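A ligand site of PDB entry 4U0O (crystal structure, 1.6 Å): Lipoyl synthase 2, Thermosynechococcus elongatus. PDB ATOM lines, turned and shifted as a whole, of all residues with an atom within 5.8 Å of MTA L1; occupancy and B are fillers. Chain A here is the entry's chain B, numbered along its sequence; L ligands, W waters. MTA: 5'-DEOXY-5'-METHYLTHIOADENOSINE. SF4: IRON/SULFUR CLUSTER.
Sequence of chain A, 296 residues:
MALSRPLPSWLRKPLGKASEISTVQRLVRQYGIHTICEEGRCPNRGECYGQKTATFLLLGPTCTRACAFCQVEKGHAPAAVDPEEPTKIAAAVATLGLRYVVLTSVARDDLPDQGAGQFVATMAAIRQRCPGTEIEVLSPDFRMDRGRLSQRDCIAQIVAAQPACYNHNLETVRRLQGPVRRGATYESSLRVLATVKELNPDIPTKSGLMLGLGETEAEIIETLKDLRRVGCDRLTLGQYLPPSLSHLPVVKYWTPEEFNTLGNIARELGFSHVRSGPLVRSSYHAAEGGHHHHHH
The side-chain carboxylate (OE2) of Glu 171 lies within hydrogen-bond range of an oxygen (O2') of MTA L1. N1 of MTA L1 sits at hydrogen-bond distance from N of Leu 241. A nitrogen (N6) of MTA L1 lies within hydrogen-bond range of the backbone carbonyl oxygen (O) of Leu 241, 2.8 Å away. ND2 of Asn 169 is in hydrogen-bond range of O3' of MTA L1, at 3.0 Å. N6 of MTA L1 lies within hydrogen-bond range of O of Phe 69. OG of Ser 283 is bound to FE4 of SF4 L2 (1.8 Å). A sulfur (S3) of SF4 L2 sits close to the side-chain hydroxyl of Thr 55. SG of Cys 70 binds FE2 of SF4 L3 (2.3 Å).
The backbone carbonyl oxygen (O) of Glu 171 is in hydrogen-bond range of the backbone NH (N) of Met 210, 2.9 Å away. The backbone carbonyl oxygen of Gly 208 sits at hydrogen-bond distance from the backbone NH of Glu 171 (3.0 Å). The side-chain amide nitrogen (ND2) of Asn 169 is in hydrogen-bond range of the side-chain hydroxyl (OG) of Ser 282, at 2.9 Å. The backbone NH (N) of Gly 208 sits at hydrogen-bond distance from the side-chain amide oxygen (OD1) of Asn 169 (2.8 Å).
A nitrogen (N3) of MTA L1 sits close to the side-chain sulfur (SD) of Met 210 (3.4 Å). Merely in contact with MTA L1: Leu 138, Gln 239, Tyr 240, Arg 281, Ser 282 and Ser 283. Hydrophobic or aromatic side chains within 4 Å of MTA L1: Phe 69, Leu 138 and Met 210. Of the 22 residues printed, 11 come within 4 Å of MTA L1. The nearest printed residue that does not touch MTA L1 is Ile 36 (4.1 Å).
Water W2 lies within hydrogen-bond range of an oxygen (O2') of MTA L1 (2.9 Å) and the backbone NH of Ser 282 (2.9 Å). Water W4 bridges N of Gln 71 (2.9 Å) and N7 of MTA L1 (3.0 Å). Water W1 lies within hydrogen-bond range of O of Val 280 and N3 of MTA L1.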
ATOM      1  N   ILE A  36     -12.192  31.306  11.186  1.00  0.00           N
ATOM      2  CA  ILE A  36     -11.968  30.489  12.373  1.00  0.00           C
ATOM      3  C   ILE A  36     -10.476  30.200  12.277  1.00  0.00           C
ATOM      4  O   ILE A  36      -9.812  29.962  13.297  1.00  0.00           O
ATOM      5  CB  ILE A  36     -12.860  29.217  12.435  1.00  0.00           C
ATOM      6  CG1 ILE A  36     -12.710  28.519  13.785  1.00  0.00           C
ATOM      7  CG2 ILE A  36     -12.450  28.262  11.337  1.00  0.00           C
ATOM      8  CD1 ILE A  36     -13.056  29.377  14.982  1.00  0.00           C
ATOM      9  N   THR A  55     -11.414  29.082   5.950  1.00  0.00           N
ATOM     10  CA  THR A  55     -12.665  28.876   6.680  1.00  0.00           C
ATOM     11  C   THR A  55     -13.181  30.114   7.400  1.00  0.00           C
ATOM     12  O   THR A  55     -12.568  30.622   8.338  1.00  0.00           O
ATOM     13  CB  THR A  55     -12.504  27.742   7.686  1.00  0.00           C
ATOM     14  OG1 THR A  55     -12.050  26.597   6.977  1.00  0.00           O
ATOM     15  CG2 THR A  55     -13.850  27.390   8.346  1.00  0.00           C
ATOM     16  N   PHE A  69     -12.602  22.825  24.466  1.00  0.00           N
ATOM     17  CA  PHE A  69     -11.489  22.700  23.540  1.00  0.00           C
ATOM     18  C   PHE A  69     -11.322  23.897  22.610  1.00  0.00           C
ATOM     19  O   PHE A  69     -10.293  24.057  21.959  1.00  0.00           O
ATOM     20  CB  PHE A  69     -11.684  21.443  22.677  1.00  0.00           C
ATOM     21  CG  PHE A  69     -12.843  21.529  21.728  1.00  0.00           C
ATOM     22  CD1 PHE A  69     -12.695  22.133  20.490  1.00  0.00           C
ATOM     23  CD2 PHE A  69     -14.088  20.998  22.071  1.00  0.00           C
ATOM     24  CE1 PHE A  69     -13.779  22.213  19.614  1.00  0.00           C
ATOM     25  CE2 PHE A  69     -15.134  21.066  21.213  1.00  0.00           C
ATOM     26  CZ  PHE A  69     -14.979  21.685  19.973  1.00  0.00           C
ATOM     27  N   CYS A  70     -12.344  24.750  22.560  1.00  0.00           N
ATOM     28  CA  CYS A  70     -12.440  25.740  21.495  1.00  0.00           C
ATOM     29  C   CYS A  70     -11.883  27.121  21.852  1.00  0.00           C
ATOM     30  O   CYS A  70     -12.172  27.669  22.922  1.00  0.00           O
ATOM     31  CB  CYS A  70     -13.891  25.853  21.108  1.00  0.00           C
ATOM     32  SG  CYS A  70     -14.229  27.017  19.758  1.00  0.00           S
ATOM     33  N   GLN A  71     -11.124  27.687  20.931  1.00  0.00           N
ATOM     34  CA  GLN A  71     -10.402  28.932  21.177  1.00  0.00           C
ATOM     35  C   GLN A  71     -11.183  30.170  20.763  1.00  0.00           C
ATOM     36  O   GLN A  71     -10.699  31.281  20.886  1.00  0.00           O
ATOM     37  CB  GLN A  71      -9.046  28.917  20.489  1.00  0.00           C
ATOM     38  CG  GLN A  71      -8.026  27.974  21.141  1.00  0.00           C
ATOM     39  CD  GLN A  71      -6.586  28.236  20.691  1.00  0.00           C
ATOM     40  OE1 GLN A  71      -5.634  28.067  21.467  1.00  0.00           O
ATOM     41  NE2 GLN A  71      -6.409  28.639  19.423  1.00  0.00           N
ATOM     42  N   LEU A 138     -19.558  23.818   7.561  1.00  0.00           N
ATOM     43  CA  LEU A 138     -19.336  23.149   8.847  1.00  0.00           C
ATOM     44  C   LEU A 138     -20.323  23.761   9.820  1.00  0.00           C
ATOM     45  O   LEU A 138     -20.141  24.891  10.287  1.00  0.00           O
ATOM     46  CB  LEU A 138     -17.894  23.375   9.326  1.00  0.00           C
ATOM     47  CG  LEU A 138     -17.583  22.942  10.779  1.00  0.00           C
ATOM     48  CD1 LEU A 138     -17.971  21.522  11.057  1.00  0.00           C
ATOM     49  CD2 LEU A 138     -16.158  23.176  11.094  1.00  0.00           C
ATOM     50  N   ASN A 169     -19.050  18.113  13.063  1.00  0.00           N
ATOM     51  CA  ASN A 169     -18.071  17.346  13.835  1.00  0.00           C
ATOM     52  C   ASN A 169     -18.641  16.786  15.121  1.00  0.00           C
ATOM     53  O   ASN A 169     -19.196  17.472  15.955  1.00  0.00           O
ATOM     54  CB  ASN A 169     -16.846  18.179  14.102  1.00  0.00           C
ATOM     55  CG  ASN A 169     -16.068  18.488  12.840  1.00  0.00           C
ATOM     56  OD1 ASN A 169     -16.088  17.701  11.897  1.00  0.00           O
ATOM     57  ND2 ASN A 169     -15.359  19.607  12.838  1.00  0.00           N
ATOM     58  N   GLU A 171     -16.479  15.353  17.239  1.00  0.00           N
ATOM     59  CA  GLU A 171     -15.417  15.835  18.123  1.00  0.00           C
ATOM     60  C   GLU A 171     -14.793  14.769  19.017  1.00  0.00           C
ATOM     61  O   GLU A 171     -13.578  14.668  19.032  1.00  0.00           O
ATOM     62  CB  GLU A 171     -15.816  16.975  19.015  1.00  0.00           C
ATOM     63  CG  GLU A 171     -16.473  18.134  18.233  1.00  0.00           C
ATOM     64  CD  GLU A 171     -15.545  18.901  17.335  1.00  0.00           C
ATOM     65  OE1 GLU A 171     -15.976  20.013  16.837  1.00  0.00           O
ATOM     66  OE2 GLU A 171     -14.437  18.435  17.031  1.00  0.00           O
ATOM     67  N   GLY A 208     -15.392  15.031  11.892  1.00  0.00           N
ATOM     68  CA  GLY A 208     -14.052  14.891  12.429  1.00  0.00           C
ATOM     69  C   GLY A 208     -14.078  14.591  13.902  1.00  0.00           C
ATOM     70  O   GLY A 208     -15.029  14.926  14.617  1.00  0.00           O
ATOM     71  N   LEU A 209     -13.015  13.922  14.360  1.00  0.00           N
ATOM     72  CA  LEU A 209     -12.774  13.720  15.783  1.00  0.00           C
ATOM     73  C   LEU A 209     -11.391  14.326  16.128  1.00  0.00           C
ATOM     74  O   LEU A 209     -10.468  14.424  15.267  1.00  0.00           O
ATOM     75  CB  LEU A 209     -12.757  12.220  16.156  1.00  0.00           C
ATOM     76  CG  LEU A 209     -13.920  11.343  15.756  1.00  0.00           C
ATOM     77  CD1 LEU A 209     -13.597   9.876  16.115  1.00  0.00           C
ATOM     78  CD2 LEU A 209     -15.169  11.823  16.488  1.00  0.00           C
ATOM     79  N   MET A 210     -11.262  14.794  17.371  1.00  0.00           N
ATOM     80  CA  MET A 210      -9.975  15.181  17.937  1.00  0.00           C
ATOM     81  C   MET A 210      -9.544  14.038  18.892  1.00  0.00           C
ATOM     82  O   MET A 210     -10.345  13.626  19.739  1.00  0.00           O
ATOM     83  CB  MET A 210     -10.102  16.466  18.751  1.00  0.00           C
ATOM     84  CG  MET A 210     -10.521  17.718  17.926  1.00  0.00           C
ATOM     85  SD  MET A 210     -10.899  19.082  19.034  1.00  0.00           S
ATOM     86  CE  MET A 210     -12.435  18.500  19.728  1.00  0.00           C
ATOM     87  N   GLY A 238      -7.572  14.294  13.933  1.00  0.00           N
ATOM     88  CA  GLY A 238      -6.471  15.154  14.291  1.00  0.00           C
ATOM     89  C   GLY A 238      -6.230  15.108  15.791  1.00  0.00           C
ATOM     90  O   GLY A 238      -6.997  14.486  16.548  1.00  0.00           O
ATOM     91  N   GLN A 239      -5.143  15.732  16.211  1.00  0.00           N
ATOM     92  CA  GLN A 239      -4.753  15.742  17.597  1.00  0.00           C
ATOM     93  C   GLN A 239      -5.337  16.937  18.312  1.00  0.00           C
ATOM     94  O   GLN A 239      -5.223  18.070  17.822  1.00  0.00           O
ATOM     95  CB  GLN A 239      -3.207  15.738  17.711  1.00  0.00           C
ATOM     96  CG  GLN A 239      -2.673  16.006  19.101  1.00  0.00           C
ATOM     97  CD  GLN A 239      -2.712  14.739  20.003  1.00  0.00           C
ATOM     98  OE1 GLN A 239      -2.414  13.645  19.543  1.00  0.00           O
ATOM     99  NE2 GLN A 239      -3.188  14.902  21.228  1.00  0.00           N
ATOM    100  N   TYR A 240      -5.966  16.670  19.458  1.00  0.00           N
ATOM    101  CA  TYR A 240      -6.342  17.699  20.417  1.00  0.00           C
ATOM    102  C   TYR A 240      -5.138  18.485  20.917  1.00  0.00           C
ATOM    103  O   TYR A 240      -4.207  17.917  21.509  1.00  0.00           O
ATOM    104  CB  TYR A 240      -7.093  17.114  21.608  1.00  0.00           C
ATOM    105  CG  TYR A 240      -7.367  18.120  22.690  1.00  0.00           C
ATOM    106  CD1 TYR A 240      -8.088  19.273  22.408  1.00  0.00           C
ATOM    107  CD2 TYR A 240      -6.876  17.958  23.982  1.00  0.00           C
ATOM    108  CE1 TYR A 240      -8.344  20.200  23.369  1.00  0.00           C
ATOM    109  CE2 TYR A 240      -7.138  18.903  24.968  1.00  0.00           C
ATOM    110  CZ  TYR A 240      -7.874  20.045  24.630  1.00  0.00           C
ATOM    111  OH  TYR A 240      -8.186  21.005  25.558  1.00  0.00           O
ATOM    112  N   LEU A 241      -5.173  19.801  20.721  1.00  0.00           N
ATOM    113  CA  LEU A 241      -4.139  20.710  21.236  1.00  0.00           C
ATOM    114  C   LEU A 241      -4.773  21.674  22.216  1.00  0.00           C
ATOM    115  O   LEU A 241      -5.523  22.556  21.813  1.00  0.00           O
ATOM    116  CB  LEU A 241      -3.471  21.481  20.097  1.00  0.00           C
ATOM    117  CG  LEU A 241      -2.753  20.618  19.055  1.00  0.00           C
ATOM    118  CD1 LEU A 241      -2.193  21.440  17.930  1.00  0.00           C
ATOM    119  CD2 LEU A 241      -1.631  19.785  19.713  1.00  0.00           C
ATOM    120  N   PRO A 242      -4.467  21.563  23.508  1.00  0.00           N
ATOM    121  CA  PRO A 242      -5.192  22.366  24.497  1.00  0.00           C
ATOM    122  C   PRO A 242      -4.882  23.861  24.380  1.00  0.00           C
ATOM    123  O   PRO A 242      -3.709  24.220  24.320  1.00  0.00           O
ATOM    124  CB  PRO A 242      -4.660  21.818  25.824  1.00  0.00           C
ATOM    125  CG  PRO A 242      -3.329  21.319  25.510  1.00  0.00           C
ATOM    126  CD  PRO A 242      -3.448  20.699  24.157  1.00  0.00           C
ATOM    127  N   PRO A 243      -5.928  24.713  24.322  1.00  0.00           N
ATOM    128  CA  PRO A 243      -5.690  26.156  24.438  1.00  0.00           C
ATOM    129  C   PRO A 243      -5.048  26.513  25.771  1.00  0.00           C
ATOM    130  O   PRO A 243      -5.352  25.879  26.781  1.00  0.00           O
ATOM    131  CB  PRO A 243      -7.085  26.758  24.364  1.00  0.00           C
ATOM    132  CG  PRO A 243      -7.928  25.722  23.687  1.00  0.00           C
ATOM    133  CD  PRO A 243      -7.362  24.409  24.123  1.00  0.00           C
ATOM    134  N   VAL A 280      -4.185  17.706  11.489  1.00  0.00           N
ATOM    135  CA  VAL A 280      -5.456  17.698  10.722  1.00  0.00           C
ATOM    136  C   VAL A 280      -6.609  18.348  11.503  1.00  0.00           C
ATOM    137  O   VAL A 280      -6.734  18.234  12.723  1.00  0.00           O
ATOM    138  CB  VAL A 280      -5.793  16.264  10.267  1.00  0.00           C
ATOM    139  CG1 VAL A 280      -7.202  16.153   9.667  1.00  0.00           C
ATOM    140  CG2 VAL A 280      -4.774  15.771   9.277  1.00  0.00           C
ATOM    141  N   ARG A 281      -7.443  19.064  10.736  1.00  0.00           N
ATOM    142  CA  ARG A 281      -8.693  19.613  11.207  1.00  0.00           C
ATOM    143  C   ARG A 281      -9.708  19.343  10.116  1.00  0.00           C
ATOM    144  O   ARG A 281      -9.344  19.000   9.000  1.00  0.00           O
ATOM    145  CB  ARG A 281      -8.617  21.140  11.384  1.00  0.00           C
ATOM    146  CG  ARG A 281      -7.349  21.641  12.082  1.00  0.00           C
ATOM    147  CD  ARG A 281      -7.710  22.496  13.299  1.00  0.00           C
ATOM    148  NE  ARG A 281      -6.545  22.757  14.144  1.00  0.00           N
ATOM    149  CZ  ARG A 281      -6.571  23.577  15.199  1.00  0.00           C
ATOM    150  NH1 ARG A 281      -5.469  23.750  15.931  1.00  0.00           N
ATOM    151  NH2 ARG A 281      -7.687  24.219  15.524  1.00  0.00           N
ATOM    152  N   SER A 282     -11.000  19.461  10.422  1.00  0.00           N
ATOM    153  CA  SER A 282     -11.991  18.943   9.477  1.00  0.00           C
ATOM    154  C   SER A 282     -11.999  19.725   8.150  1.00  0.00           C
ATOM    155  O   SER A 282     -12.362  19.158   7.140  1.00  0.00           O
ATOM    156  CB  SER A 282     -13.410  18.856  10.118  1.00  0.00           C
ATOM    157  OG  SER A 282     -13.934  20.131  10.391  1.00  0.00           O
ATOM    158  N   SER A 283     -11.599  21.002   8.169  1.00  0.00           N
ATOM    159  CA  SER A 283     -11.445  21.799   6.935  1.00  0.00           C
ATOM    160  C   SER A 283     -10.138  21.569   6.121  1.00  0.00           C
ATOM    161  O   SER A 283     -10.001  22.076   4.983  1.00  0.00           O
ATOM    162  CB  SER A 283     -11.563  23.300   7.302  1.00  0.00           C
ATOM    163  OG  SER A 283     -10.606  23.652   8.304  1.00  0.00           O
ATOM    164  N   TYR A 284      -9.205  20.820   6.672  1.00  0.00           N
ATOM    165  CA  TYR A 284      -7.873  20.659   6.048  1.00  0.00           C
ATOM    166  C   TYR A 284      -7.938  19.801   4.773  1.00  0.00           C
ATOM    167  O   TYR A 284      -8.441  18.677   4.758  1.00  0.00           O
ATOM    168  CB  TYR A 284      -6.923  20.060   7.054  1.00  0.00           C
ATOM    169  CG  TYR A 284      -5.539  19.918   6.512  1.00  0.00           C
ATOM    170  CD1 TYR A 284      -4.742  21.021   6.334  1.00  0.00           C
ATOM    171  CD2 TYR A 284      -5.050  18.678   6.133  1.00  0.00           C
ATOM    172  CE1 TYR A 284      -3.468  20.900   5.819  1.00  0.00           C
ATOM    173  CE2 TYR A 284      -3.779  18.545   5.604  1.00  0.00           C
ATOM    174  CZ  TYR A 284      -2.999  19.658   5.446  1.00  0.00           C
ATOM    175  OH  TYR A 284      -1.727  19.525   4.916  1.00  0.00           O
HETATM  176  CS  MTA L   1     -11.804  23.045  11.240  1.00  0.00           C
HETATM  177  S5' MTA L   1     -12.089  24.317  12.373  1.00  0.00           S
HETATM  178  C5' MTA L   1     -13.150  23.627  13.642  1.00  0.00           C
HETATM  179  C4' MTA L   1     -12.696  22.264  14.101  1.00  0.00           C
HETATM  180  O4' MTA L   1     -11.235  22.228  14.379  1.00  0.00           O
HETATM  181  C2' MTA L   1     -12.496  20.885  15.959  1.00  0.00           C
HETATM  182  O2' MTA L   1     -12.894  19.602  15.436  1.00  0.00           O
HETATM  183  C3' MTA L   1     -13.391  21.937  15.352  1.00  0.00           C
HETATM  184  O3' MTA L   1     -14.767  21.517  15.084  1.00  0.00           O
HETATM  185  C1' MTA L   1     -11.113  21.304  15.529  1.00  0.00           C
HETATM  186  N9  MTA L   1     -10.509  21.946  16.606  1.00  0.00           N
HETATM  187  C8  MTA L   1     -10.947  22.979  17.317  1.00  0.00           C
HETATM  188  N7  MTA L   1     -10.159  23.253  18.350  1.00  0.00           N
HETATM  189  C5  MTA L   1      -9.212  22.323  18.359  1.00  0.00           C
HETATM  190  C6  MTA L   1      -8.093  22.051  19.196  1.00  0.00           C
HETATM  191  N6  MTA L   1      -7.854  22.898  20.344  1.00  0.00           N
HETATM  192  N1  MTA L   1      -7.317  21.017  18.857  1.00  0.00           N
HETATM  193  C2  MTA L   1      -7.559  20.205  17.787  1.00  0.00           C
HETATM  194  N3  MTA L   1      -8.596  20.435  16.959  1.00  0.00           N
HETATM  195  C4  MTA L   1      -9.417  21.448  17.244  1.00  0.00           C
HETATM  196 FE1  SF4 L   2      -6.904  25.026   6.721  1.00  0.00          FE
HETATM  197 FE2  SF4 L   2      -8.271  27.184   8.120  1.00  0.00          FE
HETATM  198 FE3  SF4 L   2      -6.952  25.449   9.723  1.00  0.00          FE
HETATM  199 FE4  SF4 L   2      -9.111  24.609   8.255  1.00  0.00          FE
HETATM  200  S1  SF4 L   2      -8.988  25.959   9.746  1.00  0.00           S
HETATM  201  S2  SF4 L   2      -7.142  23.707   8.507  1.00  0.00           S
HETATM  202  S3  SF4 L   2      -8.900  25.910   6.476  1.00  0.00           S
HETATM  203  S4  SF4 L   2      -6.211  26.567   8.054  1.00  0.00           S
HETATM  204 FE1  SF4 L   3     -18.589  25.576  18.027  1.00  0.00          FE
HETATM  205 FE2  SF4 L   3     -16.549  26.778  19.614  1.00  0.00          FE
HETATM  206 FE3  SF4 L   3     -18.366  25.133  20.763  1.00  0.00          FE
HETATM  207 FE4  SF4 L   3     -18.965  27.768  20.071  1.00  0.00          FE
HETATM  208  S1  SF4 L   3     -17.595  26.982  21.531  1.00  0.00           S
HETATM  209  S2  SF4 L   3     -20.028  25.961  19.652  1.00  0.00           S
HETATM  210  S3  SF4 L   3     -17.862  27.691  18.154  1.00  0.00           S
HETATM  211  S4  SF4 L   3     -16.944  24.674  19.152  1.00  0.00           S
HETATM  212  O   HOH W   1      -8.591  18.107  14.949  1.00  0.00           O
HETATM  213  O   HOH W   2     -11.631  18.533  13.099  1.00  0.00           O
HETATM  214  O   HOH W   3     -13.513  25.176  17.133  1.00  0.00           O
HETATM  215  O   HOH W   4      -9.810  26.183  18.860  1.00  0.00           O
